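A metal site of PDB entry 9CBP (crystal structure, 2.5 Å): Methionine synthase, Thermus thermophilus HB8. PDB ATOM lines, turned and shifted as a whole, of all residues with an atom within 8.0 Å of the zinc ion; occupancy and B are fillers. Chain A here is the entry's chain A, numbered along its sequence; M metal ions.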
ATOM      1  N   GLU A   3       3.442  29.948  -2.083  1.00  0.00           N
ATOM      2  CA  GLU A   3       3.105  29.746  -0.674  1.00  0.00           C
ATOM      3  C   GLU A   3       2.748  28.276  -0.369  1.00  0.00           C
ATOM      4  O   GLU A   3       3.248  27.770   0.647  1.00  0.00           O
ATOM      5  CB  GLU A   3       2.078  30.777  -0.173  1.00  0.00           C
ATOM      6  CG  GLU A   3       2.602  32.224  -0.099  1.00  0.00           C
ATOM      7  CD  GLU A   3       3.844  32.456   0.783  1.00  0.00           C
ATOM      8  OE1 GLU A   3       4.226  31.635   1.695  1.00  0.00           O
ATOM      9  OE2 GLU A   3       4.496  33.497   0.473  1.00  0.00           O
ATOM     10  N   VAL A   4       1.996  27.568  -1.261  1.00  0.00           N
ATOM     11  CA  VAL A   4       1.656  26.133  -1.128  1.00  0.00           C
ATOM     12  C   VAL A   4       2.895  25.280  -0.805  1.00  0.00           C
ATOM     13  O   VAL A   4       2.810  24.378   0.013  1.00  0.00           O
ATOM     14  CB  VAL A   4       0.869  25.510  -2.325  1.00  0.00           C
ATOM     15  CG1 VAL A   4      -0.494  26.153  -2.556  1.00  0.00           C
ATOM     16  CG2 VAL A   4       1.652  25.528  -3.647  1.00  0.00           C
ATOM     17  N   HIS A   5       4.066  25.608  -1.395  1.00  0.00           N
ATOM     18  CA  HIS A   5       5.313  24.880  -1.184  1.00  0.00           C
ATOM     19  C   HIS A   5       6.133  25.390   0.004  1.00  0.00           C
ATOM     20  O   HIS A   5       7.113  24.739   0.365  1.00  0.00           O
ATOM     21  CB  HIS A   5       6.191  24.923  -2.455  1.00  0.00           C
ATOM     22  CG  HIS A   5       5.588  24.195  -3.607  1.00  0.00           C
ATOM     23  ND1 HIS A   5       4.814  24.821  -4.558  1.00  0.00           N
ATOM     24  CD2 HIS A   5       5.593  22.900  -3.919  1.00  0.00           C
ATOM     25  CE1 HIS A   5       4.354  23.924  -5.425  1.00  0.00           C
ATOM     26  NE2 HIS A   5       4.805  22.754  -5.047  1.00  0.00           N
ATOM     27  N   ALA A   6       5.745  26.519   0.647  1.00  0.00           N
ATOM     28  CA  ALA A   6       6.570  27.173   1.671  1.00  0.00           C
ATOM     29  C   ALA A   6       6.123  26.827   3.101  1.00  0.00           C
ATOM     30  O   ALA A   6       6.492  27.503   4.039  1.00  0.00           O
ATOM     31  CB  ALA A   6       6.531  28.651   1.401  1.00  0.00           C
ATOM     32  N   CYS A   7       5.398  25.740   3.316  1.00  0.00           N
ATOM     33  CA  CYS A   7       5.128  25.258   4.670  1.00  0.00           C
ATOM     34  C   CYS A   7       6.349  24.656   5.373  1.00  0.00           C
ATOM     35  O   CYS A   7       7.164  24.017   4.712  1.00  0.00           O
ATOM     36  CB  CYS A   7       4.067  24.180   4.662  1.00  0.00           C
ATOM     37  SG  CYS A   7       2.414  24.830   4.366  1.00  0.00           S
ATOM     38  N   SER A   8       6.423  24.805   6.706  1.00  0.00           N
ATOM     39  CA  SER A   8       7.286  24.004   7.569  1.00  0.00           C
ATOM     40  C   SER A   8       6.476  22.860   8.156  1.00  0.00           C
ATOM     41  O   SER A   8       5.249  22.913   8.051  1.00  0.00           O
ATOM     42  CB  SER A   8       7.916  24.793   8.653  1.00  0.00           C
ATOM     43  OG  SER A   8       7.019  25.135   9.682  1.00  0.00           O
ATOM     44  N   PRO A   9       7.084  21.822   8.787  1.00  0.00           N
ATOM     45  CA  PRO A   9       6.325  20.835   9.569  1.00  0.00           C
ATOM     46  C   PRO A   9       5.559  21.396  10.783  1.00  0.00           C
ATOM     47  O   PRO A   9       4.829  20.645  11.435  1.00  0.00           O
ATOM     48  CB  PRO A   9       7.403  19.873  10.098  1.00  0.00           C
ATOM     49  CG  PRO A   9       8.548  20.035   9.165  1.00  0.00           C
ATOM     50  CD  PRO A   9       8.519  21.485   8.720  1.00  0.00           C
ATOM     51  N   GLY A  10       5.708  22.702  11.112  1.00  0.00           N
ATOM     52  CA  GLY A  10       4.979  23.337  12.212  1.00  0.00           C
ATOM     53  C   GLY A  10       3.563  23.833  11.851  1.00  0.00           C
ATOM     54  O   GLY A  10       2.765  23.997  12.762  1.00  0.00           O
ATOM     55  N   CYS A  11       3.312  24.176  10.569  1.00  0.00           N
ATOM     56  CA  CYS A  11       2.047  24.576  10.008  1.00  0.00           C
ATOM     57  C   CYS A  11       0.949  23.544  10.232  1.00  0.00           C
ATOM     58  O   CYS A  11       1.089  22.347   9.950  1.00  0.00           O
ATOM     59  CB  CYS A  11       2.273  24.747   8.516  1.00  0.00           C
ATOM     60  SG  CYS A  11       3.291  26.134   7.932  1.00  0.00           S
ATOM     61  N   ARG A  12      -0.092  24.112  10.786  1.00  0.00           N
ATOM     62  CA  ARG A  12      -1.395  23.477  10.861  1.00  0.00           C
ATOM     63  C   ARG A  12      -2.428  24.459  10.309  1.00  0.00           C
ATOM     64  O   ARG A  12      -2.851  25.401  10.952  1.00  0.00           O
ATOM     65  CB  ARG A  12      -1.721  23.101  12.292  1.00  0.00           C
ATOM     66  CG  ARG A  12      -0.722  22.179  12.973  1.00  0.00           C
ATOM     67  CD  ARG A  12      -0.955  20.719  12.431  1.00  0.00           C
ATOM     68  NE  ARG A  12       0.011  19.797  13.043  1.00  0.00           N
ATOM     69  CZ  ARG A  12       1.338  19.706  12.819  1.00  0.00           C
ATOM     70  NH1 ARG A  12       1.936  20.363  11.849  1.00  0.00           N
ATOM     71  NH2 ARG A  12       2.033  18.872  13.552  1.00  0.00           N
ATOM     72  N   HIS A  13      -2.740  24.260   9.064  1.00  0.00           N
ATOM     73  CA  HIS A  13      -3.671  25.125   8.372  1.00  0.00           C
ATOM     74  C   HIS A  13      -5.070  24.523   8.208  1.00  0.00           C
ATOM     75  O   HIS A  13      -5.871  25.116   7.519  1.00  0.00           O
ATOM     76  CB  HIS A  13      -3.163  25.351   6.965  1.00  0.00           C
ATOM     77  CG  HIS A  13      -1.865  26.109   6.975  1.00  0.00           C
ATOM     78  ND1 HIS A  13      -1.488  26.941   8.019  1.00  0.00           N
ATOM     79  CD2 HIS A  13      -0.842  26.033   6.120  1.00  0.00           C
ATOM     80  CE1 HIS A  13      -0.287  27.444   7.713  1.00  0.00           C
ATOM     81  NE2 HIS A  13       0.112  26.836   6.577  1.00  0.00           N
ATOM     82  N   GLY A  17      -7.239  27.769   8.224  1.00  0.00           N
ATOM     83  CA  GLY A  17      -6.833  28.084   6.847  1.00  0.00           C
ATOM     84  C   GLY A  17      -5.482  28.802   6.812  1.00  0.00           C
ATOM     85  O   GLY A  17      -4.931  29.199   7.858  1.00  0.00           O
ATOM     86  N   ALA A  18      -4.934  28.862   5.597  1.00  0.00           N
ATOM     87  CA  ALA A  18      -3.681  29.548   5.413  1.00  0.00           C
ATOM     88  C   ALA A  18      -3.953  30.974   4.867  1.00  0.00           C
ATOM     89  O   ALA A  18      -5.048  31.556   5.021  1.00  0.00           O
ATOM     90  CB  ALA A  18      -2.803  28.631   4.603  1.00  0.00           C
ATOM     91  N   GLY A  19      -2.941  31.592   4.213  1.00  0.00           N
ATOM     92  CA  GLY A  19      -3.063  32.946   3.706  1.00  0.00           C
ATOM     93  C   GLY A  19      -3.533  33.062   2.264  1.00  0.00           C
ATOM     94  O   GLY A  19      -3.633  34.186   1.807  1.00  0.00           O
ATOM     95  N   TRP A  20      -3.778  31.937   1.585  1.00  0.00           N
ATOM     96  CA  TRP A  20      -4.170  31.896   0.164  1.00  0.00           C
ATOM     97  C   TRP A  20      -5.469  31.100  -0.043  1.00  0.00           C
ATOM     98  O   TRP A  20      -6.059  30.520   0.887  1.00  0.00           O
ATOM     99  CB  TRP A  20      -3.015  31.338  -0.679  1.00  0.00           C
ATOM    100  CG  TRP A  20      -2.659  29.909  -0.367  1.00  0.00           C
ATOM    101  CD1 TRP A  20      -3.181  28.792  -0.971  1.00  0.00           C
ATOM    102  CD2 TRP A  20      -1.740  29.413   0.613  1.00  0.00           C
ATOM    103  NE1 TRP A  20      -2.684  27.659  -0.393  1.00  0.00           N
ATOM    104  CE2 TRP A  20      -1.786  28.001   0.570  1.00  0.00           C
ATOM    105  CE3 TRP A  20      -0.891  30.021   1.533  1.00  0.00           C
ATOM    106  CZ2 TRP A  20      -1.013  27.180   1.368  1.00  0.00           C
ATOM    107  CZ3 TRP A  20      -0.137  29.199   2.316  1.00  0.00           C
ATOM    108  CH2 TRP A  20      -0.165  27.807   2.238  1.00  0.00           C
ATOM    109  N   ASP A 476       5.752  28.794  13.181  1.00  0.00           N
ATOM    110  CA  ASP A 476       4.613  28.345  12.377  1.00  0.00           C
ATOM    111  C   ASP A 476       3.541  27.659  13.232  1.00  0.00           C
ATOM    112  O   ASP A 476       2.344  27.823  12.948  1.00  0.00           O
ATOM    113  CB  ASP A 476       5.069  27.494  11.184  1.00  0.00           C
ATOM    114  CG  ASP A 476       5.650  28.283  10.008  1.00  0.00           C
ATOM    115  OD1 ASP A 476       5.334  29.524   9.888  1.00  0.00           O
ATOM    116  OD2 ASP A 476       6.471  27.683   9.266  1.00  0.00           O
ATOM    117  N   SER A 480       0.031  29.271  13.556  1.00  0.00           N
ATOM    118  CA  SER A 480      -1.086  28.427  13.204  1.00  0.00           C
ATOM    119  C   SER A 480      -2.152  28.406  14.298  1.00  0.00           C
ATOM    120  O   SER A 480      -3.370  28.343  14.025  1.00  0.00           O
ATOM    121  CB  SER A 480      -0.618  27.003  12.937  1.00  0.00           C
ATOM    122  OG  SER A 480      -0.081  26.868  11.635  1.00  0.00           O
ATOM    123  N   ARG A 516       5.589  36.415   6.669  1.00  0.00           N
ATOM    124  CA  ARG A 516       5.207  35.035   6.981  1.00  0.00           C
ATOM    125  C   ARG A 516       3.832  34.963   7.667  1.00  0.00           C
ATOM    126  O   ARG A 516       3.023  34.111   7.371  1.00  0.00           O
ATOM    127  CB  ARG A 516       6.335  34.447   7.830  1.00  0.00           C
ATOM    128  CG  ARG A 516       6.185  32.971   8.191  1.00  0.00           C
ATOM    129  CD  ARG A 516       6.305  32.079   7.005  1.00  0.00           C
ATOM    130  NE  ARG A 516       6.215  30.649   7.323  1.00  0.00           N
ATOM    131  CZ  ARG A 516       6.265  29.699   6.407  1.00  0.00           C
ATOM    132  NH1 ARG A 516       6.475  30.029   5.153  1.00  0.00           N
ATOM    133  NH2 ARG A 516       6.253  28.446   6.723  1.00  0.00           N
ATOM    134  N   HIS A 520       1.657  34.031   4.371  1.00  0.00           N
ATOM    135  CA  HIS A 520       1.620  32.581   4.463  1.00  0.00           C
ATOM    136  C   HIS A 520       0.478  32.083   5.356  1.00  0.00           C
ATOM    137  O   HIS A 520      -0.173  31.089   5.014  1.00  0.00           O
ATOM    138  CB  HIS A 520       2.961  32.063   4.968  1.00  0.00           C
ATOM    139  CG  HIS A 520       3.088  30.592   4.852  1.00  0.00           C
ATOM    140  ND1 HIS A 520       3.433  30.041   3.625  1.00  0.00           N
ATOM    141  CD2 HIS A 520       2.989  29.587   5.723  1.00  0.00           C
ATOM    142  CE1 HIS A 520       3.597  28.735   3.785  1.00  0.00           C
ATOM    143  NE2 HIS A 520       3.227  28.390   5.035  1.00  0.00           N
ATOM    144  N   HIS A 521       0.287  32.693   6.526  1.00  0.00           N
ATOM    145  CA  HIS A 521      -0.653  32.202   7.508  1.00  0.00           C
ATOM    146  C   HIS A 521      -2.038  32.872   7.431  1.00  0.00           C
ATOM    147  O   HIS A 521      -3.036  32.246   7.823  1.00  0.00           O
ATOM    148  CB  HIS A 521      -0.085  32.372   8.906  1.00  0.00           C
ATOM    149  CG  HIS A 521       0.953  31.364   9.252  1.00  0.00           C
ATOM    150  ND1 HIS A 521       0.641  30.051   9.513  1.00  0.00           N
ATOM    151  CD2 HIS A 521       2.325  31.497   9.377  1.00  0.00           C
ATOM    152  CE1 HIS A 521       1.785  29.408   9.800  1.00  0.00           C
ATOM    153  NE2 HIS A 521       2.833  30.299   9.762  1.00  0.00           N
HETATM  154 ZN    ZN M   1       2.210  26.604   6.007  1.00  0.00          ZN
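The backbone NH of Ser 8 lies close to the side-chain sulfur of Cys 11, 3.6 Å away. SG of Cys 11 lies close to OD2 of Asp 476 (3.8 Å). ND1 of His 520 is in hydrogen-bond range of NH1 of Arg 516, 3.4 Å away. ND1 of His 520 lies within hydrogen-bond range of OE1 of Glu 3 (2.6 Å). The backbone NH of Gly 19 lies within hydrogen-bond range of the backbone carbonyl oxygen of His 520, 2.9 Å away.
A ring nitrogen (NE2) of His 13 binds the zinc ion (2.2 Å). The zinc ion is bound by the side-chain sulfur (SG) of Cys 11 (2.3 Å). The zinc ion is bound by NE2 of His 520 (2.3 Å). SG of Cys 7 binds the zinc ion (2.4 Å).
Within 4 Å of the zinc ion: Cys 7, Cys 11, His 13 and His 520.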
